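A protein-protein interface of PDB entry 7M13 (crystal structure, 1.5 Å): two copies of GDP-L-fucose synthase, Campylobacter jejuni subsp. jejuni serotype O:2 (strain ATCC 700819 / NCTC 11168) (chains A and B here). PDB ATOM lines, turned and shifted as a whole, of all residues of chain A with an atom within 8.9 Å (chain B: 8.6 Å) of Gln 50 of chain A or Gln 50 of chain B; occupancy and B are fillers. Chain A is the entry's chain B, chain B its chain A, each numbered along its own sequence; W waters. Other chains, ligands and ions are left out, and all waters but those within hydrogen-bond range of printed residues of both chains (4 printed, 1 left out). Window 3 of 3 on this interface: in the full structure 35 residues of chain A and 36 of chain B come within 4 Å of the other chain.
The backbone carbonyl oxygen of Val 47 of chain B lies close to the side-chain amide oxygen of Gln 49 of chain A (3.2 Å).
The side-chain amide nitrogen (NE2) of Gln 49 of chain B is in hydrogen-bond range of the backbone carbonyl oxygen (O) of Val 47 of chain A, at 3.2 Å.
NE2 of Gln 49 of chain A lies close to N of Gln 49 of chain B (2.8 Å).
The side-chain hydroxyl (OH) of Tyr 85 of chain A sits at hydrogen-bond distance from the side-chain amide nitrogen (NE2) of Gln 49 of chain B (3.3 Å).
O of Val 47 of chain B lies within hydrogen-bond range of ND2 of Asn 93 of chain B, 3.1 Å away.
The side-chain amide oxygen of Asn 48 of chain B is in hydrogen-bond range of the backbone NH of Gln 50 of chain B (3.3 Å).
O of Val 47 of chain A is in hydrogen-bond range of ND2 of Asn 93 of chain A (3.1 Å).
OD1 of Asn 48 of chain A sits at hydrogen-bond distance from N of Ala 51 of chain A (2.8 Å).
The backbone NH (N) of Gln 49 of chain A lies close to the side-chain amide nitrogen (ND2) of Asn 93 of chain A, 3.4 Å away.
CA of Asn 48 of chain A touches OE1 of Gln 49 of chain B (3.4 Å).
Gln 49 of chain A touches Asn 48 of chain B.
OE1 of Gln 49 of chain A touches CE of Met 89 of chain B (3.4 Å).
Gln 50 of chain A touches Gln 50 of chain B.
Met 89 of chain A touches Gln 49 of chain B.
Met 89 of chain B touches Met 89 of chain A.
Gln 50 of chain A touches just one residue of chain B: Gln 50 (3.4 Å).
Of chain A, only Gln 50 comes within 4 Å of Gln 50 of chain B.
Ala 51 of chain A touches none of the printed residues of chain B.
No residue of chain A comes within 4 Å of Ala 51 of chain B.
Printed residues of chain A within 4 Å of Gln 49 of chain B: Val 47, Asn 48, Gln 49, Tyr 85 and Met 89.
Of the printed residues of chain A, Val 47 of chain B touches Gln 49.
Of the printed residues of chain B, Tyr 85 of chain A touches Gln 49.
Phe 56 of chain A touches none of the printed residues of chain B.
The nearest residue of chain A that does not touch Gln 50 of chain B is Gln 49 of chain A (4.4 Å).
Of the 18 printed residues of chain B, 5 touch a printed residue of chain A.
Along chain B the printed residues that touch a printed residue of chain A span positions 47 to 89.
Of the 18 printed residues of chain A, 6 touch a printed residue of chain B.
Printed residues of chain A that touch a printed residue of chain B: Val 47, Asn 48, Gln 49, Gln 50, Tyr 85 and Met 89.
Among the printed residues, 10 pairs touch across the chains.
Among the printed residues, no Asp or Glu carboxylate lies within 4 Å of a Lys or Arg side-chain nitrogen of the other chain.
Asn 48 of chain A touches Gln 49 of chain B, and with the chains exchanged Gln 49 of chain A touches Asn 48 of chain B.
Gln 49 of chain B touches its own counterpart, Gln 49 of chain A.
Gln 49 of chain A touches Met 89 of chain B, and with the chains exchanged Met 89 of chain A touches Gln 49 of chain B.
Positions printed for both chains: 44, 45, 46, 47, 48, 49, 50, 51, 52, 53, 54, 55, 56, 57, 89, 93 and 97.
Of the 10 pairs that touch across the chains among the printed residues, 9 have their exchanged pair printed and touching as well.
Water W4 lies within hydrogen-bond range of the side-chain hydroxyl of Tyr 85 of chain A and the side-chain amide nitrogen of Gln 49 of chain B.
Water W1 lies within hydrogen-bond range of OH of Tyr 85 of chain A, OD1 of Asn 93 of chain B, ND2 of Asn 97 of chain B and NE2 of Gln 49 of chain B.
Water W3 bridges the side-chain amide nitrogen of Gln 50 of chain A (3.0 Å) and the side-chain amide nitrogen of Gln 50 of chain B (3.3 Å).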
ATOM      1  N   LEU A  44      -1.011 -11.383 -16.254  1.00  0.00           N
ATOM      2  CA  LEU A  44      -1.012  -9.954 -16.651  1.00  0.00           C
ATOM      3  C   LEU A  44      -0.735  -9.864 -18.153  1.00  0.00           C
ATOM      4  O   LEU A  44       0.392 -10.149 -18.607  1.00  0.00           O
ATOM      5  CB  LEU A  44       0.031  -9.180 -15.840  1.00  0.00           C
ATOM      6  CG  LEU A  44       0.268  -7.710 -16.211  1.00  0.00           C
ATOM      7  CD1 LEU A  44      -1.008  -6.907 -16.070  1.00  0.00           C
ATOM      8  CD2 LEU A  44       1.389  -7.155 -15.352  1.00  0.00           C
ATOM      9  N   ASP A  45      -1.769  -9.546 -18.919  1.00  0.00           N
ATOM     10  CA  ASP A  45      -1.655  -9.297 -20.371  1.00  0.00           C
ATOM     11  C   ASP A  45      -1.159  -7.866 -20.576  1.00  0.00           C
ATOM     12  O   ASP A  45      -1.916  -6.925 -20.304  1.00  0.00           O
ATOM     13  CB  ASP A  45      -3.000  -9.499 -21.046  1.00  0.00           C
ATOM     14  CG  ASP A  45      -2.957  -9.247 -22.548  1.00  0.00           C
ATOM     15  OD1 ASP A  45      -1.839  -9.005 -23.139  1.00  0.00           O
ATOM     16  OD2 ASP A  45      -4.057  -9.297 -23.160  1.00  0.00           O
ATOM     17  N   LEU A  46       0.105  -7.682 -20.985  1.00  0.00           N
ATOM     18  CA  LEU A  46       0.732  -6.337 -21.015  1.00  0.00           C
ATOM     19  C   LEU A  46       0.177  -5.461 -22.162  1.00  0.00           C
ATOM     20  O   LEU A  46       0.429  -4.247 -22.116  1.00  0.00           O
ATOM     21  CB  LEU A  46       2.246  -6.498 -21.170  1.00  0.00           C
ATOM     22  CG  LEU A  46       2.925  -7.063 -19.915  1.00  0.00           C
ATOM     23  CD1 LEU A  46       4.380  -7.317 -20.211  1.00  0.00           C
ATOM     24  CD2 LEU A  46       2.774  -6.118 -18.766  1.00  0.00           C
ATOM     25  N   VAL A  47      -0.607  -6.034 -23.071  1.00  0.00           N
ATOM     26  CA  VAL A  47      -1.322  -5.253 -24.112  1.00  0.00           C
ATOM     27  C   VAL A  47      -2.519  -4.537 -23.480  1.00  0.00           C
ATOM     28  O   VAL A  47      -3.022  -3.601 -24.103  1.00  0.00           O
ATOM     29  CB  VAL A  47      -1.689  -6.149 -25.303  1.00  0.00           C
ATOM     30  CG1 VAL A  47      -2.605  -5.462 -26.301  1.00  0.00           C
ATOM     31  CG2 VAL A  47      -0.428  -6.644 -25.994  1.00  0.00           C
ATOM     32  N   ASN A  48      -3.033  -5.041 -22.361  1.00  0.00           N
ATOM     33  CA  ASN A  48      -4.284  -4.532 -21.776  1.00  0.00           C
ATOM     34  C   ASN A  48      -3.967  -3.399 -20.801  1.00  0.00           C
ATOM     35  O   ASN A  48      -3.428  -3.653 -19.714  1.00  0.00           O
ATOM     36  CB  ASN A  48      -5.071  -5.686 -21.142  1.00  0.00           C
ATOM     37  CG  ASN A  48      -6.429  -5.237 -20.635  1.00  0.00           C
ATOM     38  OD1 ASN A  48      -6.519  -4.765 -19.524  1.00  0.00           O
ATOM     39  ND2 ASN A  48      -7.445  -5.231 -21.500  1.00  0.00           N
ATOM     40  N   GLN A  49      -4.287  -2.182 -21.192  1.00  0.00           N
ATOM     41  CA  GLN A  49      -4.020  -0.979 -20.408  1.00  0.00           C
ATOM     42  C   GLN A  49      -4.633  -1.078 -19.016  1.00  0.00           C
ATOM     43  O   GLN A  49      -3.952  -0.799 -18.044  1.00  0.00           O
ATOM     44  CB  GLN A  49      -4.541   0.211 -21.194  1.00  0.00           C
ATOM     45  CG  GLN A  49      -4.393   1.488 -20.414  1.00  0.00           C
ATOM     46  CD  GLN A  49      -5.011   2.645 -21.145  1.00  0.00           C
ATOM     47  OE1 GLN A  49      -4.353   3.628 -21.498  1.00  0.00           O
ATOM     48  NE2 GLN A  49      -6.288   2.534 -21.344  1.00  0.00           N
ATOM     49  N   GLN A  50      -5.885  -1.530 -18.914  1.00  0.00           N
ATOM     50  CA  GLN A  50      -6.567  -1.621 -17.607  1.00  0.00           C
ATOM     51  C   GLN A  50      -5.769  -2.552 -16.685  1.00  0.00           C
ATOM     52  O   GLN A  50      -5.547  -2.178 -15.534  1.00  0.00           O
ATOM     53  CB  GLN A  50      -8.001  -2.091 -17.814  1.00  0.00           C
ATOM     54  CG  GLN A  50      -8.780  -2.217 -16.516  1.00  0.00           C
ATOM     55  CD  GLN A  50     -10.170  -2.773 -16.727  1.00  0.00           C
ATOM     56  OE1 GLN A  50     -10.551  -3.246 -17.800  1.00  0.00           O
ATOM     57  NE2 GLN A  50     -10.953  -2.709 -15.669  1.00  0.00           N
ATOM     58  N   ALA A  51      -5.385  -3.715 -17.172  1.00  0.00           N
ATOM     59  CA  ALA A  51      -4.685  -4.689 -16.296  1.00  0.00           C
ATOM     60  C   ALA A  51      -3.321  -4.116 -15.883  1.00  0.00           C
ATOM     61  O   ALA A  51      -2.836  -4.323 -14.744  1.00  0.00           O
ATOM     62  CB  ALA A  51      -4.536  -6.000 -16.998  1.00  0.00           C
ATOM     63  N   VAL A  52      -2.614  -3.464 -16.807  1.00  0.00           N
ATOM     64  CA  VAL A  52      -1.270  -2.929 -16.495  1.00  0.00           C
ATOM     65  C   VAL A  52      -1.381  -1.780 -15.486  1.00  0.00           C
ATOM     66  O   VAL A  52      -0.602  -1.735 -14.518  1.00  0.00           O
ATOM     67  CB  VAL A  52      -0.521  -2.527 -17.771  1.00  0.00           C
ATOM     68  CG1 VAL A  52       0.779  -1.844 -17.394  1.00  0.00           C
ATOM     69  CG2 VAL A  52      -0.269  -3.741 -18.628  1.00  0.00           C
ATOM     70  N   ALA A  53      -2.361  -0.892 -15.645  1.00  0.00           N
ATOM     71  CA  ALA A  53      -2.558   0.204 -14.705  1.00  0.00           C
ATOM     72  C   ALA A  53      -2.847  -0.379 -13.310  1.00  0.00           C
ATOM     73  O   ALA A  53      -2.285   0.106 -12.333  1.00  0.00           O
ATOM     74  CB  ALA A  53      -3.656   1.079 -15.246  1.00  0.00           C
ATOM     75  N   LYS A  54      -3.701  -1.391 -13.231  1.00  0.00           N
ATOM     76  CA  LYS A  54      -4.043  -2.017 -11.928  1.00  0.00           C
ATOM     77  C   LYS A  54      -2.800  -2.639 -11.293  1.00  0.00           C
ATOM     78  O   LYS A  54      -2.593  -2.498 -10.071  1.00  0.00           O
ATOM     79  CB  LYS A  54      -5.086  -3.121 -12.111  1.00  0.00           C
ATOM     80  CG  LYS A  54      -6.522  -2.656 -12.222  1.00  0.00           C
ATOM     81  CD  LYS A  54      -7.465  -3.831 -12.239  1.00  0.00           C
ATOM     82  CE  LYS A  54      -8.923  -3.433 -12.331  1.00  0.00           C
ATOM     83  NZ  LYS A  54      -9.726  -4.540 -12.904  1.00  0.00           N
ATOM     84  N   PHE A  55      -1.986  -3.333 -12.083  1.00  0.00           N
ATOM     85  CA  PHE A  55      -0.745  -3.970 -11.584  1.00  0.00           C
ATOM     86  C   PHE A  55       0.170  -2.923 -10.948  1.00  0.00           C
ATOM     87  O   PHE A  55       0.723  -3.127  -9.853  1.00  0.00           O
ATOM     88  CB  PHE A  55      -0.009  -4.713 -12.701  1.00  0.00           C
ATOM     89  CG  PHE A  55       1.418  -5.056 -12.388  1.00  0.00           C
ATOM     90  CD1 PHE A  55       1.708  -6.119 -11.548  1.00  0.00           C
ATOM     91  CD2 PHE A  55       2.455  -4.251 -12.834  1.00  0.00           C
ATOM     92  CE1 PHE A  55       3.015  -6.447 -11.244  1.00  0.00           C
ATOM     93  CE2 PHE A  55       3.760  -4.544 -12.482  1.00  0.00           C
ATOM     94  CZ  PHE A  55       4.037  -5.627 -11.679  1.00  0.00           C
ATOM     95  N   PHE A  56       0.439  -1.818 -11.648  1.00  0.00           N
ATOM     96  CA  PHE A  56       1.356  -0.784 -11.132  1.00  0.00           C
ATOM     97  C   PHE A  56       0.810  -0.149  -9.860  1.00  0.00           C
ATOM     98  O   PHE A  56       1.582   0.074  -8.911  1.00  0.00           O
ATOM     99  CB  PHE A  56       1.685   0.255 -12.203  1.00  0.00           C
ATOM    100  CG  PHE A  56       2.846  -0.165 -13.065  1.00  0.00           C
ATOM    101  CD1 PHE A  56       4.145   0.123 -12.686  1.00  0.00           C
ATOM    102  CD2 PHE A  56       2.652  -0.875 -14.236  1.00  0.00           C
ATOM    103  CE1 PHE A  56       5.206  -0.328 -13.454  1.00  0.00           C
ATOM    104  CE2 PHE A  56       3.703  -1.279 -15.033  1.00  0.00           C
ATOM    105  CZ  PHE A  56       4.986  -1.012 -14.618  1.00  0.00           C
ATOM    106  N   LYS A  57      -0.502   0.085  -9.804  1.00  0.00           N
ATOM    107  CA  LYS A  57      -1.127   0.719  -8.614  1.00  0.00           C
ATOM    108  C   LYS A  57      -1.074  -0.261  -7.433  1.00  0.00           C
ATOM    109  O   LYS A  57      -0.844   0.199  -6.291  1.00  0.00           O
ATOM    110  CB  LYS A  57      -2.557   1.157  -8.968  1.00  0.00           C
ATOM    111  CG  LYS A  57      -3.129   2.284  -8.106  1.00  0.00           C
ATOM    112  CD  LYS A  57      -2.374   3.605  -8.192  1.00  0.00           C
ATOM    113  CE  LYS A  57      -2.432   4.315  -9.533  1.00  0.00           C
ATOM    114  NZ  LYS A  57      -1.931   5.711  -9.444  1.00  0.00           N
ATOM    115  N   TYR A  85       1.223  -2.982 -33.368  1.00  0.00           N
ATOM    116  CA  TYR A  85       0.205  -2.761 -32.318  1.00  0.00           C
ATOM    117  C   TYR A  85       0.650  -3.330 -30.959  1.00  0.00           C
ATOM    118  O   TYR A  85       0.573  -2.620 -29.943  1.00  0.00           O
ATOM    119  CB  TYR A  85      -1.145  -3.314 -32.758  1.00  0.00           C
ATOM    120  CG  TYR A  85      -2.185  -3.238 -31.673  1.00  0.00           C
ATOM    121  CD1 TYR A  85      -2.724  -2.025 -31.279  1.00  0.00           C
ATOM    122  CD2 TYR A  85      -2.556  -4.344 -30.958  1.00  0.00           C
ATOM    123  CE1 TYR A  85      -3.652  -1.921 -30.253  1.00  0.00           C
ATOM    124  CE2 TYR A  85      -3.475  -4.270 -29.923  1.00  0.00           C
ATOM    125  CZ  TYR A  85      -4.037  -3.052 -29.571  1.00  0.00           C
ATOM    126  OH  TYR A  85      -4.928  -2.978 -28.531  1.00  0.00           O
ATOM    127  N   MET A  89       1.591  -1.210 -27.615  1.00  0.00           N
ATOM    128  CA  MET A  89       0.743  -1.277 -26.414  1.00  0.00           C
ATOM    129  C   MET A  89       1.585  -1.694 -25.189  1.00  0.00           C
ATOM    130  O   MET A  89       1.440  -1.054 -24.135  1.00  0.00           O
ATOM    131  CB  MET A  89      -0.457  -2.201 -26.568  1.00  0.00           C
ATOM    132  CG  MET A  89      -1.504  -1.708 -27.610  1.00  0.00           C
ATOM    133  SD  MET A  89      -2.205  -0.099 -27.208  1.00  0.00           S
ATOM    134  CE  MET A  89      -2.834  -0.452 -25.577  1.00  0.00           C
ATOM    135  N   ASN A  93       1.949   0.998 -22.297  1.00  0.00           N
ATOM    136  CA  ASN A  93       1.309   0.655 -21.006  1.00  0.00           C
ATOM    137  C   ASN A  93       2.361   0.605 -19.892  1.00  0.00           C
ATOM    138  O   ASN A  93       2.130   1.179 -18.816  1.00  0.00           O
ATOM    139  CB  ASN A  93       0.578  -0.672 -21.116  1.00  0.00           C
ATOM    140  CG  ASN A  93      -0.686  -0.630 -21.961  1.00  0.00           C
ATOM    141  OD1 ASN A  93      -1.248   0.436 -22.181  1.00  0.00           O
ATOM    142  ND2 ASN A  93      -1.098  -1.806 -22.409  1.00  0.00           N
ATOM    143  N   ASN A  97       2.570   3.799 -17.211  1.00  0.00           N
ATOM    144  CA  ASN A  97       2.145   3.404 -15.842  1.00  0.00           C
ATOM    145  C   ASN A  97       3.338   3.375 -14.891  1.00  0.00           C
ATOM    146  O   ASN A  97       3.152   3.675 -13.720  1.00  0.00           O
ATOM    147  CB  ASN A  97       1.291   2.144 -15.839  1.00  0.00           C
ATOM    148  CG  ASN A  97      -0.069   2.486 -16.407  1.00  0.00           C
ATOM    149  OD1 ASN A  97      -0.856   3.167 -15.727  1.00  0.00           O
ATOM    150  ND2 ASN A  97      -0.289   2.193 -17.685  1.00  0.00           N
ATOM    151  N   LEU B  44     -16.146  10.033 -24.005  1.00  0.00           N
ATOM    152  CA  LEU B  44     -15.284   8.929 -24.487  1.00  0.00           C
ATOM    153  C   LEU B  44     -13.851   9.446 -24.546  1.00  0.00           C
ATOM    154  O   LEU B  44     -13.528  10.249 -25.447  1.00  0.00           O
ATOM    155  CB  LEU B  44     -15.747   8.431 -25.856  1.00  0.00           C
ATOM    156  CG  LEU B  44     -14.847   7.380 -26.533  1.00  0.00           C
ATOM    157  CD1 LEU B  44     -14.681   6.141 -25.667  1.00  0.00           C
ATOM    158  CD2 LEU B  44     -15.376   7.013 -27.905  1.00  0.00           C
ATOM    159  N   ASP B  45     -13.027   9.035 -23.575  1.00  0.00           N
ATOM    160  CA  ASP B  45     -11.594   9.408 -23.575  1.00  0.00           C
ATOM    161  C   ASP B  45     -10.841   8.441 -24.484  1.00  0.00           C
ATOM    162  O   ASP B  45     -10.720   7.262 -24.139  1.00  0.00           O
ATOM    163  CB  ASP B  45     -11.044   9.280 -22.163  1.00  0.00           C
ATOM    164  CG  ASP B  45      -9.578   9.591 -22.026  1.00  0.00           C
ATOM    165  OD1 ASP B  45      -8.930   9.989 -23.019  1.00  0.00           O
ATOM    166  OD2 ASP B  45      -9.100   9.447 -20.867  1.00  0.00           O
ATOM    167  N   LEU B  46     -10.362   8.928 -25.632  1.00  0.00           N
ATOM    168  CA  LEU B  46      -9.801   8.007 -26.667  1.00  0.00           C
ATOM    169  C   LEU B  46      -8.403   7.501 -26.265  1.00  0.00           C
ATOM    170  O   LEU B  46      -7.945   6.553 -26.911  1.00  0.00           O
ATOM    171  CB  LEU B  46      -9.721   8.741 -28.001  1.00  0.00           C
ATOM    172  CG  LEU B  46     -11.066   9.114 -28.622  1.00  0.00           C
ATOM    173  CD1 LEU B  46     -10.896  10.041 -29.812  1.00  0.00           C
ATOM    174  CD2 LEU B  46     -11.850   7.882 -28.972  1.00  0.00           C
ATOM    175  N   VAL B  47      -7.802   8.015 -25.203  1.00  0.00           N
ATOM    176  CA  VAL B  47      -6.569   7.409 -24.616  1.00  0.00           C
ATOM    177  C   VAL B  47      -6.905   6.125 -23.841  1.00  0.00           C
ATOM    178  O   VAL B  47      -6.029   5.301 -23.645  1.00  0.00           O
ATOM    179  CB  VAL B  47      -5.828   8.477 -23.790  1.00  0.00           C
ATOM    180  CG1 VAL B  47      -4.691   7.904 -22.956  1.00  0.00           C
ATOM    181  CG2 VAL B  47      -5.312   9.556 -24.716  1.00  0.00           C
ATOM    182  N   ASN B  48      -8.161   5.956 -23.394  1.00  0.00           N
ATOM    183  CA  ASN B  48      -8.551   4.835 -22.518  1.00  0.00           C
ATOM    184  C   ASN B  48      -9.007   3.659 -23.383  1.00  0.00           C
ATOM    185  O   ASN B  48     -10.089   3.709 -24.017  1.00  0.00           O
ATOM    186  CB  ASN B  48      -9.599   5.296 -21.523  1.00  0.00           C
ATOM    187  CG  ASN B  48      -9.947   4.207 -20.530  1.00  0.00           C
ATOM    188  OD1 ASN B  48     -10.782   3.336 -20.808  1.00  0.00           O
ATOM    189  ND2 ASN B  48      -9.185   4.145 -19.443  1.00  0.00           N
ATOM    190  N   GLN B  49      -8.182   2.637 -23.461  1.00  0.00           N
ATOM    191  CA  GLN B  49      -8.469   1.435 -24.252  1.00  0.00           C
ATOM    192  C   GLN B  49      -9.823   0.835 -23.874  1.00  0.00           C
ATOM    193  O   GLN B  49     -10.558   0.436 -24.808  1.00  0.00           O
ATOM    194  CB  GLN B  49      -7.326   0.456 -24.025  1.00  0.00           C
ATOM    195  CG  GLN B  49      -7.495  -0.828 -24.796  1.00  0.00           C
ATOM    196  CD  GLN B  49      -6.456  -1.845 -24.425  1.00  0.00           C
ATOM    197  OE1 GLN B  49      -6.282  -2.184 -23.260  1.00  0.00           O
ATOM    198  NE2 GLN B  49      -5.710  -2.333 -25.399  1.00  0.00           N
ATOM    199  N   GLN B  50     -10.105   0.684 -22.588  1.00  0.00           N
ATOM    200  CA  GLN B  50     -11.341   0.004 -22.126  1.00  0.00           C
ATOM    201  C   GLN B  50     -12.550   0.755 -22.694  1.00  0.00           C
ATOM    202  O   GLN B  50     -13.457   0.117 -23.218  1.00  0.00           O
ATOM    203  CB  GLN B  50     -11.334  -0.065 -20.611  1.00  0.00           C
ATOM    204  CG  GLN B  50     -12.586  -0.683 -20.047  1.00  0.00           C
ATOM    205  CD  GLN B  50     -12.603  -0.645 -18.537  1.00  0.00           C
ATOM    206  OE1 GLN B  50     -11.797   0.030 -17.875  1.00  0.00           O
ATOM    207  NE2 GLN B  50     -13.568  -1.345 -17.974  1.00  0.00           N
ATOM    208  N   ALA B  51     -12.560   2.063 -22.584  1.00  0.00           N
ATOM    209  CA  ALA B  51     -13.698   2.891 -23.044  1.00  0.00           C
ATOM    210  C   ALA B  51     -13.821   2.815 -24.563  1.00  0.00           C
ATOM    211  O   ALA B  51     -14.945   2.725 -25.092  1.00  0.00           O
ATOM    212  CB  ALA B  51     -13.568   4.293 -22.581  1.00  0.00           C
ATOM    213  N   VAL B  52     -12.700   2.857 -25.302  1.00  0.00           N
ATOM    214  CA  VAL B  52     -12.773   2.802 -26.790  1.00  0.00           C
ATOM    215  C   VAL B  52     -13.248   1.417 -27.245  1.00  0.00           C
ATOM    216  O   VAL B  52     -14.054   1.341 -28.177  1.00  0.00           O
ATOM    217  CB  VAL B  52     -11.422   3.192 -27.428  1.00  0.00           C
ATOM    218  CG1 VAL B  52     -11.463   3.045 -28.943  1.00  0.00           C
ATOM    219  CG2 VAL B  52     -11.055   4.625 -27.068  1.00  0.00           C
ATOM    220  N   ALA B  53     -12.797   0.334 -26.619  1.00  0.00           N
ATOM    221  CA  ALA B  53     -13.148  -1.038 -27.040  1.00  0.00           C
ATOM    222  C   ALA B  53     -14.647  -1.211 -26.809  1.00  0.00           C
ATOM    223  O   ALA B  53     -15.300  -1.796 -27.686  1.00  0.00           O
ATOM    224  CB  ALA B  53     -12.347  -1.981 -26.194  1.00  0.00           C
ATOM    225  N   LYS B  54     -15.131  -0.641 -25.707  1.00  0.00           N
ATOM    226  CA  LYS B  54     -16.579  -0.716 -25.338  1.00  0.00           C
ATOM    227  C   LYS B  54     -17.382   0.047 -26.403  1.00  0.00           C
ATOM    228  O   LYS B  54     -18.425  -0.490 -26.880  1.00  0.00           O
ATOM    229  CB  LYS B  54     -16.872  -0.168 -23.945  1.00  0.00           C
ATOM    230  CG  LYS B  54     -18.333  -0.286 -23.533  1.00  0.00           C
ATOM    231  CD  LYS B  54     -18.553   0.264 -22.147  1.00  0.00           C
ATOM    232  CE  LYS B  54     -20.020   0.365 -21.771  1.00  0.00           C
ATOM    233  NZ  LYS B  54     -20.606  -0.965 -21.484  1.00  0.00           N
ATOM    234  N   PHE B  55     -16.977   1.272 -26.731  1.00  0.00           N
ATOM    235  CA  PHE B  55     -17.672   2.103 -27.747  1.00  0.00           C
ATOM    236  C   PHE B  55     -17.805   1.323 -29.032  1.00  0.00           C
ATOM    237  O   PHE B  55     -18.901   1.284 -29.634  1.00  0.00           O
ATOM    238  CB  PHE B  55     -16.945   3.429 -27.948  1.00  0.00           C
ATOM    239  CG  PHE B  55     -17.429   4.175 -29.156  1.00  0.00           C
ATOM    240  CD1 PHE B  55     -18.605   4.883 -29.110  1.00  0.00           C
ATOM    241  CD2 PHE B  55     -16.686   4.200 -30.308  1.00  0.00           C
ATOM    242  CE1 PHE B  55     -19.058   5.554 -30.227  1.00  0.00           C
ATOM    243  CE2 PHE B  55     -17.150   4.862 -31.430  1.00  0.00           C
ATOM    244  CZ  PHE B  55     -18.331   5.536 -31.379  1.00  0.00           C
ATOM    245  N   PHE B  56     -16.724   0.753 -29.560  1.00  0.00           N
ATOM    246  CA  PHE B  56     -16.782   0.040 -30.849  1.00  0.00           C
ATOM    247  C   PHE B  56     -17.666  -1.212 -30.746  1.00  0.00           C
ATOM    248  O   PHE B  56     -18.439  -1.472 -31.661  1.00  0.00           O
ATOM    249  CB  PHE B  56     -15.382  -0.273 -31.351  1.00  0.00           C
ATOM    250  CG  PHE B  56     -14.741   0.840 -32.120  1.00  0.00           C
ATOM    251  CD1 PHE B  56     -15.032   1.029 -33.453  1.00  0.00           C
ATOM    252  CD2 PHE B  56     -13.975   1.801 -31.464  1.00  0.00           C
ATOM    253  CE1 PHE B  56     -14.462   2.078 -34.145  1.00  0.00           C
ATOM    254  CE2 PHE B  56     -13.423   2.864 -32.149  1.00  0.00           C
ATOM    255  CZ  PHE B  56     -13.703   3.014 -33.484  1.00  0.00           C
ATOM    256  N   LYS B  57     -17.573  -1.971 -29.663  1.00  0.00           N
ATOM    257  CA  LYS B  57     -18.410  -3.187 -29.500  1.00  0.00           C
ATOM    258  C   LYS B  57     -19.886  -2.814 -29.424  1.00  0.00           C
ATOM    259  O   LYS B  57     -20.710  -3.619 -29.926  1.00  0.00           O
ATOM    260  CB  LYS B  57     -18.030  -3.970 -28.237  1.00  0.00           C
ATOM    261  CG  LYS B  57     -16.830  -4.888 -28.389  1.00  0.00           C
ATOM    262  CD  LYS B  57     -17.097  -6.141 -29.193  1.00  0.00           C
ATOM    263  CE  LYS B  57     -15.816  -6.843 -29.592  1.00  0.00           C
ATOM    264  NZ  LYS B  57     -16.117  -8.142 -30.237  1.00  0.00           N
ATOM    265  N   GLU B  58     -20.211  -1.696 -28.784  1.00  0.00           N
ATOM    266  CA  GLU B  58     -21.632  -1.374 -28.457  1.00  0.00           C
ATOM    267  C   GLU B  58     -22.268  -0.491 -29.538  1.00  0.00           C
ATOM    268  O   GLU B  58     -23.529  -0.491 -29.594  1.00  0.00           O
ATOM    269  CB  GLU B  58     -21.713  -0.801 -27.066  1.00  0.00           C
ATOM    270  CG  GLU B  58     -21.436  -1.917 -26.063  1.00  0.00           C
ATOM    271  CD  GLU B  58     -21.638  -1.653 -24.590  1.00  0.00           C
ATOM    272  OE1 GLU B  58     -22.303  -0.676 -24.257  1.00  0.00           O
ATOM    273  OE2 GLU B  58     -21.074  -2.445 -23.775  1.00  0.00           O
ATOM    274  N   MET B  89      -1.723   6.365 -28.207  1.00  0.00           N
ATOM    275  CA  MET B  89      -2.864   5.650 -27.586  1.00  0.00           C
ATOM    276  C   MET B  89      -4.148   5.883 -28.404  1.00  0.00           C
ATOM    277  O   MET B  89      -4.911   4.922 -28.624  1.00  0.00           O
ATOM    278  CB  MET B  89      -3.069   6.094 -26.135  1.00  0.00           C
ATOM    279  CG  MET B  89      -2.034   5.572 -25.154  1.00  0.00           C
ATOM    280  SD  MET B  89      -1.733   3.819 -25.182  1.00  0.00           S
ATOM    281  CE  MET B  89      -3.344   3.232 -24.675  1.00  0.00           C
ATOM    282  N   ASN B  93      -5.813   2.765 -30.131  1.00  0.00           N
ATOM    283  CA  ASN B  93      -7.130   2.329 -29.632  1.00  0.00           C
ATOM    284  C   ASN B  93      -8.141   2.382 -30.769  1.00  0.00           C
ATOM    285  O   ASN B  93      -8.962   1.439 -30.918  1.00  0.00           O
ATOM    286  CB  ASN B  93      -7.606   3.182 -28.475  1.00  0.00           C
ATOM    287  CG  ASN B  93      -6.835   2.944 -27.196  1.00  0.00           C
ATOM    288  OD1 ASN B  93      -6.263   1.877 -27.012  1.00  0.00           O
ATOM    289  ND2 ASN B  93      -6.834   3.938 -26.304  1.00  0.00           N
ATOM    290  N   ASN B  97      -9.393  -1.171 -32.517  1.00  0.00           N
ATOM    291  CA  ASN B  97     -10.806  -1.542 -32.190  1.00  0.00           C
ATOM    292  C   ASN B  97     -11.654  -1.408 -33.452  1.00  0.00           C
ATOM    293  O   ASN B  97     -12.695  -2.060 -33.564  1.00  0.00           O
ATOM    294  CB  ASN B  97     -11.317  -0.782 -30.981  1.00  0.00           C
ATOM    295  CG  ASN B  97     -10.664  -1.377 -29.752  1.00  0.00           C
ATOM    296  OD1 ASN B  97     -11.055  -2.436 -29.295  1.00  0.00           O
ATOM    297  ND2 ASN B  97      -9.610  -0.750 -29.230  1.00  0.00           N
HETATM  298  O   HOH W   1      -6.784  -0.819 -28.067  1.00  0.00           O
HETATM  299  O   HOH W   2      -8.164   0.879 -20.393  1.00  0.00           O
HETATM  300  O   HOH W   3     -13.854  -2.902 -15.108  1.00  0.00           O
HETATM  301  O   HOH W   4      -6.350  -4.967 -27.534  1.00  0.00           O
